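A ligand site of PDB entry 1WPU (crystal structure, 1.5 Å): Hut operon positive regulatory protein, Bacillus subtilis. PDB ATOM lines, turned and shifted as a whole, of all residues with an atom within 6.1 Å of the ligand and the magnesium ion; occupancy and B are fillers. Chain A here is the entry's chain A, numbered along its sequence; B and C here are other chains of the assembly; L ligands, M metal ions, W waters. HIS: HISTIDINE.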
ATOM      1  N   VAL A  85      19.557  11.983  23.234  1.00  0.00           N
ATOM      2  CA  VAL A  85      19.921  10.971  24.203  1.00  0.00           C
ATOM      3  C   VAL A  85      20.781   9.870  23.603  1.00  0.00           C
ATOM      4  O   VAL A  85      21.770   9.449  24.205  1.00  0.00           O
ATOM      5  CB  VAL A  85      18.662  10.346  24.846  1.00  0.00           C
ATOM      6  CG1 VAL A  85      19.045   9.117  25.688  1.00  0.00           C
ATOM      7  CG2 VAL A  85      17.952  11.380  25.701  1.00  0.00           C
ATOM      8  N   THR A  86      20.408   9.397  22.415  1.00  0.00           N
ATOM      9  CA  THR A  86      21.125   8.302  21.765  1.00  0.00           C
ATOM     10  C   THR A  86      22.275   8.698  20.848  1.00  0.00           C
ATOM     11  O   THR A  86      23.169   7.893  20.573  1.00  0.00           O
ATOM     12  CB  THR A  86      20.156   7.389  21.000  1.00  0.00           C
ATOM     13  OG1 THR A  86      19.431   8.160  20.039  1.00  0.00           O
ATOM     14  CG2 THR A  86      19.156   6.744  21.967  1.00  0.00           C
ATOM     15  N   ARG A  87      22.250   9.931  20.339  1.00  0.00           N
ATOM     16  CA  ARG A  87      23.323  10.457  19.492  1.00  0.00           C
ATOM     17  C   ARG A  87      23.849   9.603  18.335  1.00  0.00           C
ATOM     18  O   ARG A  87      25.047   9.296  18.295  1.00  0.00           O
ATOM     19  CB  ARG A  87      24.488  10.882  20.385  1.00  0.00           C
ATOM     20  CG  ARG A  87      24.199  12.087  21.266  1.00  0.00           C
ATOM     21  CD  ARG A  87      24.885  11.984  22.624  1.00  0.00           C
ATOM     22  NE  ARG A  87      24.364  10.832  23.354  1.00  0.00           N
ATOM     23  CZ  ARG A  87      25.106   9.837  23.822  1.00  0.00           C
ATOM     24  NH1 ARG A  87      26.428   9.844  23.664  1.00  0.00           N
ATOM     25  NH2 ARG A  87      24.528   8.799  24.414  1.00  0.00           N
ATOM     26  N   LEU A  95      22.662  -2.183  21.762  1.00  0.00           N
ATOM     27  CA  LEU A  95      24.038  -1.692  21.700  1.00  0.00           C
ATOM     28  C   LEU A  95      24.675  -1.747  23.079  1.00  0.00           C
ATOM     29  O   LEU A  95      25.594  -0.999  23.398  1.00  0.00           O
ATOM     30  CB  LEU A  95      24.084  -0.263  21.150  1.00  0.00           C
ATOM     31  CG  LEU A  95      23.673  -0.096  19.687  1.00  0.00           C
ATOM     32  CD1 LEU A  95      23.937   1.352  19.277  1.00  0.00           C
ATOM     33  CD2 LEU A  95      24.448  -1.044  18.793  1.00  0.00           C
ATOM     34  N   LEU A  96      24.172  -2.653  23.908  1.00  0.00           N
ATOM     35  CA  LEU A  96      24.672  -2.869  25.258  1.00  0.00           C
ATOM     36  C   LEU A  96      24.713  -1.633  26.140  1.00  0.00           C
ATOM     37  O   LEU A  96      25.684  -1.374  26.838  1.00  0.00           O
ATOM     38  CB  LEU A  96      26.077  -3.514  25.191  1.00  0.00           C
ATOM     39  CG  LEU A  96      26.482  -4.325  26.419  1.00  0.00           C
ATOM     40  CD1 LEU A  96      25.453  -5.421  26.689  1.00  0.00           C
ATOM     41  CD2 LEU A  96      27.859  -4.931  26.197  1.00  0.00           C
ATOM     42  N   ARG A  97      23.634  -0.845  26.103  1.00  0.00           N
ATOM     43  CA  ARG A  97      23.555   0.321  26.969  1.00  0.00           C
ATOM     44  C   ARG A  97      22.154   0.466  27.526  1.00  0.00           C
ATOM     45  O   ARG A  97      21.184  -0.045  26.970  1.00  0.00           O
ATOM     46  CB  ARG A  97      24.024   1.595  26.255  1.00  0.00           C
ATOM     47  CG  ARG A  97      23.213   2.033  25.073  1.00  0.00           C
ATOM     48  CD  ARG A  97      23.846   3.260  24.418  1.00  0.00           C
ATOM     49  NE  ARG A  97      23.110   3.624  23.213  1.00  0.00           N
ATOM     50  CZ  ARG A  97      23.393   4.679  22.443  1.00  0.00           C
ATOM     51  NH1 ARG A  97      24.399   5.491  22.742  1.00  0.00           N
ATOM     52  NH2 ARG A  97      22.672   4.891  21.348  1.00  0.00           N
ATOM     53  N   THR A  98      22.087   1.169  28.648  1.00  0.00           N
ATOM     54  CA  THR A  98      20.837   1.386  29.362  1.00  0.00           C
ATOM     55  C   THR A  98      20.703   2.851  29.747  1.00  0.00           C
ATOM     56  O   THR A  98      21.712   3.558  29.886  1.00  0.00           O
ATOM     57  CB  THR A  98      20.845   0.520  30.645  1.00  0.00           C
ATOM     58  OG1 THR A  98      19.736   0.855  31.481  1.00  0.00           O
ATOM     59  CG2 THR A  98      22.148   0.728  31.415  1.00  0.00           C
ATOM     60  N   ILE A 128      23.209   7.513  30.827  1.00  0.00           N
ATOM     61  CA  ILE A 128      23.247   6.432  29.847  1.00  0.00           C
ATOM     62  C   ILE A 128      24.591   5.734  30.068  1.00  0.00           C
ATOM     63  O   ILE A 128      25.576   6.385  30.379  1.00  0.00           O
ATOM     64  CB  ILE A 128      23.121   6.983  28.388  1.00  0.00           C
ATOM     65  CG1 ILE A 128      22.977   5.821  27.413  1.00  0.00           C
ATOM     66  CG2 ILE A 128      24.340   7.828  28.039  1.00  0.00           C
ATOM     67  CD1 ILE A 128      22.514   6.280  26.032  1.00  0.00           C
ATOM     68  N   GLY A 129      24.617   4.416  29.934  1.00  0.00           N
ATOM     69  CA  GLY A 129      25.874   3.724  30.125  1.00  0.00           C
ATOM     70  C   GLY A 129      25.789   2.219  29.959  1.00  0.00           C
ATOM     71  O   GLY A 129      24.797   1.692  29.461  1.00  0.00           O
ATOM     72  N   ALA A 130      26.853   1.536  30.364  1.00  0.00           N
ATOM     73  CA  ALA A 130      26.900   0.088  30.299  1.00  0.00           C
ATOM     74  C   ALA A 130      25.963  -0.410  31.381  1.00  0.00           C
ATOM     75  O   ALA A 130      25.654   0.319  32.338  1.00  0.00           O
ATOM     76  CB  ALA A 130      28.317  -0.389  30.560  1.00  0.00           C
ATOM     77  N   PRO A 131      25.494  -1.662  31.263  1.00  0.00           N
ATOM     78  CA  PRO A 131      24.577  -2.239  32.256  1.00  0.00           C
ATOM     79  C   PRO A 131      25.272  -2.572  33.581  1.00  0.00           C
ATOM     80  O   PRO A 131      25.149  -3.687  34.071  1.00  0.00           O
ATOM     81  CB  PRO A 131      24.053  -3.500  31.556  1.00  0.00           C
ATOM     82  CG  PRO A 131      24.298  -3.240  30.098  1.00  0.00           C
ATOM     83  CD  PRO A 131      25.622  -2.552  30.111  1.00  0.00           C
ATOM     84  N   LEU A 135      29.050   2.902  35.616  1.00  0.00           N
ATOM     85  CA  LEU A 135      29.694   3.002  34.305  1.00  0.00           C
ATOM     86  C   LEU A 135      28.714   3.731  33.398  1.00  0.00           C
ATOM     87  O   LEU A 135      28.121   3.154  32.487  1.00  0.00           O
ATOM     88  CB  LEU A 135      29.986   1.608  33.744  1.00  0.00           C
ATOM     89  CG  LEU A 135      30.826   0.698  34.648  1.00  0.00           C
ATOM     90  CD1 LEU A 135      31.197  -0.566  33.871  1.00  0.00           C
ATOM     91  CD2 LEU A 135      32.086   1.406  35.119  1.00  0.00           C
ATOM     92  N   GLU A 136      28.570   5.028  33.655  1.00  0.00           N
ATOM     93  CA  GLU A 136      27.609   5.833  32.919  1.00  0.00           C
ATOM     94  C   GLU A 136      27.967   7.320  32.989  1.00  0.00           C
ATOM     95  O   GLU A 136      28.792   7.741  33.798  1.00  0.00           O
ATOM     96  CB  GLU A 136      26.234   5.637  33.575  1.00  0.00           C
ATOM     97  CG  GLU A 136      26.154   6.231  34.993  1.00  0.00           C
ATOM     98  CD  GLU A 136      25.206   5.489  35.926  1.00  0.00           C
ATOM     99  OE1 GLU A 136      24.585   6.146  36.790  1.00  0.00           O
ATOM    100  OE2 GLU A 136      25.096   4.250  35.839  1.00  0.00           O
ATOM    101  N   HIS A 137      27.347   8.093  32.104  1.00  0.00           N
ATOM    102  CA  HIS A 137      27.501   9.541  32.111  1.00  0.00           C
ATOM    103  C   HIS A 137      26.143  10.145  31.794  1.00  0.00           C
ATOM    104  O   HIS A 137      25.197   9.429  31.448  1.00  0.00           O
ATOM    105  CB  HIS A 137      28.622  10.044  31.163  1.00  0.00           C
ATOM    106  CG  HIS A 137      28.437   9.705  29.722  1.00  0.00           C
ATOM    107  ND1 HIS A 137      27.387  10.207  28.967  1.00  0.00           N
ATOM    108  CD2 HIS A 137      29.202   8.992  28.870  1.00  0.00           C
ATOM    109  CE1 HIS A 137      27.526   9.807  27.714  1.00  0.00           C
ATOM    110  NE2 HIS A 137      28.621   9.065  27.635  1.00  0.00           N
ATOM    111  N   TYR B  68      35.339   3.755  34.863  1.00  0.00           N
ATOM    112  CA  TYR B  68      34.558   3.948  33.637  1.00  0.00           C
ATOM    113  C   TYR B  68      35.363   4.496  32.463  1.00  0.00           C
ATOM    114  O   TYR B  68      35.158   4.071  31.327  1.00  0.00           O
ATOM    115  CB  TYR B  68      33.384   4.894  33.918  1.00  0.00           C
ATOM    116  CG  TYR B  68      32.431   5.094  32.761  1.00  0.00           C
ATOM    117  CD1 TYR B  68      31.983   3.999  32.016  1.00  0.00           C
ATOM    118  CD2 TYR B  68      31.933   6.358  32.446  1.00  0.00           C
ATOM    119  CE1 TYR B  68      31.055   4.158  30.990  1.00  0.00           C
ATOM    120  CE2 TYR B  68      30.994   6.525  31.425  1.00  0.00           C
ATOM    121  CZ  TYR B  68      30.569   5.422  30.702  1.00  0.00           C
ATOM    122  OH  TYR B  68      29.628   5.568  29.707  1.00  0.00           O
ATOM    123  N   SER B  71      36.664   2.104  29.830  1.00  0.00           N
ATOM    124  CA  SER B  71      35.569   1.349  29.244  1.00  0.00           C
ATOM    125  C   SER B  71      34.813   2.283  28.298  1.00  0.00           C
ATOM    126  O   SER B  71      34.333   1.857  27.246  1.00  0.00           O
ATOM    127  CB  SER B  71      34.609   0.853  30.333  1.00  0.00           C
ATOM    128  OG  SER B  71      35.215  -0.158  31.114  1.00  0.00           O
ATOM    129  N   HIS B  72      34.732   3.551  28.670  1.00  0.00           N
ATOM    130  CA  HIS B  72      34.061   4.553  27.849  1.00  0.00           C
ATOM    131  C   HIS B  72      34.810   4.712  26.524  1.00  0.00           C
ATOM    132  O   HIS B  72      34.198   4.738  25.453  1.00  0.00           O
ATOM    133  CB  HIS B  72      34.019   5.899  28.567  1.00  0.00           C
ATOM    134  CG  HIS B  72      33.218   6.932  27.841  1.00  0.00           C
ATOM    135  ND1 HIS B  72      33.788   7.942  27.083  1.00  0.00           N
ATOM    136  CD2 HIS B  72      31.877   7.088  27.708  1.00  0.00           C
ATOM    137  CE1 HIS B  72      32.837   8.669  26.528  1.00  0.00           C
ATOM    138  NE2 HIS B  72      31.665   8.166  26.888  1.00  0.00           N
ATOM    139  N   TYR B  75      34.261   1.562  24.395  1.00  0.00           N
ATOM    140  CA  TYR B  75      32.915   1.466  23.848  1.00  0.00           C
ATOM    141  C   TYR B  75      32.764   2.308  22.586  1.00  0.00           C
ATOM    142  O   TYR B  75      32.253   1.843  21.570  1.00  0.00           O
ATOM    143  CB  TYR B  75      31.879   1.889  24.891  1.00  0.00           C
ATOM    144  CG  TYR B  75      30.453   1.802  24.400  1.00  0.00           C
ATOM    145  CD1 TYR B  75      29.806   2.908  23.854  1.00  0.00           C
ATOM    146  CD2 TYR B  75      29.757   0.595  24.452  1.00  0.00           C
ATOM    147  CE1 TYR B  75      28.493   2.814  23.372  1.00  0.00           C
ATOM    148  CE2 TYR B  75      28.461   0.483  23.973  1.00  0.00           C
ATOM    149  CZ  TYR B  75      27.835   1.598  23.436  1.00  0.00           C
ATOM    150  OH  TYR B  75      26.541   1.493  22.989  1.00  0.00           O
ATOM    151  N   HIS B  76      33.220   3.548  22.636  1.00  0.00           N
ATOM    152  CA  HIS B  76      33.089   4.417  21.470  1.00  0.00           C
ATOM    153  C   HIS B  76      33.974   3.972  20.308  1.00  0.00           C
ATOM    154  O   HIS B  76      33.577   4.119  19.159  1.00  0.00           O
ATOM    155  CB  HIS B  76      33.348   5.852  21.884  1.00  0.00           C
ATOM    156  CG  HIS B  76      32.174   6.462  22.589  1.00  0.00           C
ATOM    157  ND1 HIS B  76      31.038   6.856  21.922  1.00  0.00           N
ATOM    158  CD2 HIS B  76      31.939   6.674  23.899  1.00  0.00           C
ATOM    159  CE1 HIS B  76      30.143   7.285  22.797  1.00  0.00           C
ATOM    160  NE2 HIS B  76      30.662   7.185  24.005  1.00  0.00           N
ATOM    161  N   GLU C  80      28.579  15.064  19.394  1.00  0.00           N
ATOM    162  CA  GLU C  80      27.479  14.496  20.156  1.00  0.00           C
ATOM    163  C   GLU C  80      26.439  15.557  20.511  1.00  0.00           C
ATOM    164  O   GLU C  80      25.245  15.299  20.447  1.00  0.00           O
ATOM    165  CB  GLU C  80      28.010  13.802  21.417  1.00  0.00           C
ATOM    166  CG  GLU C  80      28.700  12.473  21.114  1.00  0.00           C
ATOM    167  CD  GLU C  80      28.946  11.636  22.350  1.00  0.00           C
ATOM    168  OE1 GLU C  80      28.440  12.020  23.424  1.00  0.00           O
ATOM    169  N   TRP C 119      36.713  15.075  32.361  1.00  0.00           N
ATOM    170  CA  TRP C 119      35.710  14.836  31.336  1.00  0.00           C
ATOM    171  C   TRP C 119      35.322  16.194  30.809  1.00  0.00           C
ATOM    172  O   TRP C 119      35.623  17.218  31.423  1.00  0.00           O
ATOM    173  CB  TRP C 119      34.488  14.127  31.933  1.00  0.00           C
ATOM    174  CG  TRP C 119      34.787  12.711  32.290  1.00  0.00           C
ATOM    175  CD1 TRP C 119      35.648  12.271  33.246  1.00  0.00           C
ATOM    176  CD2 TRP C 119      34.279  11.540  31.640  1.00  0.00           C
ATOM    177  NE1 TRP C 119      35.708  10.904  33.237  1.00  0.00           N
ATOM    178  CE2 TRP C 119      34.880  10.426  32.259  1.00  0.00           C
ATOM    179  CE3 TRP C 119      33.377  11.326  30.586  1.00  0.00           C
ATOM    180  CZ2 TRP C 119      34.606   9.110  31.881  1.00  0.00           C
ATOM    181  CZ3 TRP C 119      33.107  10.018  30.204  1.00  0.00           C
ATOM    182  CH2 TRP C 119      33.726   8.924  30.848  1.00  0.00           C
ATOM    183  N   ILE C 144      29.049  14.620  25.964  1.00  0.00           N
ATOM    184  CA  ILE C 144      29.974  14.377  27.074  1.00  0.00           C
ATOM    185  C   ILE C 144      31.057  13.379  26.630  1.00  0.00           C
ATOM    186  O   ILE C 144      30.757  12.393  25.978  1.00  0.00           O
ATOM    187  CB  ILE C 144      29.213  13.817  28.300  1.00  0.00           C
ATOM    188  CG1 ILE C 144      28.267  14.899  28.851  1.00  0.00           C
ATOM    189  CG2 ILE C 144      30.191  13.377  29.396  1.00  0.00           C
ATOM    190  CD1 ILE C 144      27.388  14.451  29.992  1.00  0.00           C
ATOM    191  N   ASN C 145      32.311  13.650  26.991  1.00  0.00           N
ATOM    192  CA  ASN C 145      33.406  12.771  26.601  1.00  0.00           C
ATOM    193  C   ASN C 145      34.503  12.805  27.650  1.00  0.00           C
ATOM    194  O   ASN C 145      34.564  13.723  28.464  1.00  0.00           O
ATOM    195  CB  ASN C 145      33.960  13.235  25.241  1.00  0.00           C
ATOM    196  CG  ASN C 145      34.672  12.132  24.497  1.00  0.00           C
ATOM    197  OD1 ASN C 145      34.603  10.953  24.867  1.00  0.00           O
ATOM    198  ND2 ASN C 145      35.359  12.489  23.417  1.00  0.00           N
HETATM  199  CA  HIS L   1      27.948   5.481  25.870  1.00  0.00           C
HETATM  200  C   HIS L   1      27.107   6.597  25.265  1.00  0.00           C
HETATM  201  O   HIS L   1      27.637   7.700  25.077  1.00  0.00           O
HETATM  202  CB  HIS L   1      27.118   4.614  26.809  1.00  0.00           C
HETATM  203  CG  HIS L   1      27.860   3.386  27.270  1.00  0.00           C
HETATM  204  ND1 HIS L   1      28.927   3.453  28.131  1.00  0.00           N
HETATM  205  CD2 HIS L   1      27.737   2.086  26.903  1.00  0.00           C
HETATM  206  CE1 HIS L   1      29.442   2.247  28.272  1.00  0.00           C
HETATM  207  NE2 HIS L   1      28.738   1.400  27.536  1.00  0.00           N
HETATM  208  OXT HIS L   1      25.927   6.358  24.966  1.00  0.00           O
HETATM  209 MG    MG M   1      29.617   8.105  25.831  1.00  0.00          MG
HETATM  210  O   HOH W   1      31.437  -0.537  28.821  1.00  0.00           O
HETATM  211  O   HOH W   2      28.371  -1.440  27.411  1.00  0.00           O
HETATM  212  O   HOH W   3      29.849  10.040  24.874  1.00  0.00           O
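The nearest printed residue that does not touch the magnesium ion is Arg 87 (4.2 Å).
The magnesium ion is bound by an oxygen (O) of the ligand (2.2 Å), water W3 (2.2 Å), a ring nitrogen (NE2) of His 137 (2.3 Å), a ring nitrogen (NE2) of His 76 of chain B (2.3 Å) and a ring nitrogen (NE2) of His 72 of chain B (2.3 Å). The magnesium ion has five donor atoms within binding distance.
Water W3 lies within hydrogen-bond range of O of Ile 144 of chain C (2.8 Å) and OE1 of Glu 80 of chain C (2.8 Å). Water W2 bridges O of Leu 96 (2.7 Å) and NE2 of the ligand (2.9 Å).
The backbone NH (N) of Ile 128 sits at hydrogen-bond distance from the backbone carbonyl oxygen (O) of His 137, at 2.8 Å. The backbone carbonyl oxygen of Thr 86 is in hydrogen-bond range of the guanidinium group of Arg 97 (3.1 Å). The side-chain carboxylate (OE1) of Glu 80 of chain C lies within salt-bridge range of the guanidinium group (NH1) of Arg 87 (3.0 Å). O of Val 85 is in hydrogen-bond range of NH2 of Arg 87, 2.8 Å away. The backbone carbonyl oxygen of Leu 95 sits at hydrogen-bond distance from the side-chain hydroxyl of Tyr 75 of chain B, at 2.7 Å. The backbone NH of Ala 130 sits at hydrogen-bond distance from the backbone carbonyl oxygen of Leu 135, at 3.0 Å. The backbone NH (N) of Thr 98 is in hydrogen-bond range of the backbone carbonyl oxygen (O) of Gly 129, at 2.9 Å.
Merely in contact with the ligand: Ile 128, Gly 129 and Tyr 75 of chain B. Hydrophobic or aromatic side chains that line the ligand: Ile 128, Ala 130, His 137, Tyr 68 of chain B, Tyr 75 of chain B and His 76 of chain B.
A nitrogen (ND1) of the ligand is in hydrogen-bond range of the side-chain hydroxyl of Tyr 68 of chain B. NH1 of Arg 97 is in salt-bridge range of OXT of the ligand, 2.8 Å away. OXT of the ligand lies within salt-bridge range of NH2 of Arg 87 (2.9 Å). A nitrogen (NE2) of the ligand sits close to the backbone NH of Ala 130, 3.4 Å away.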
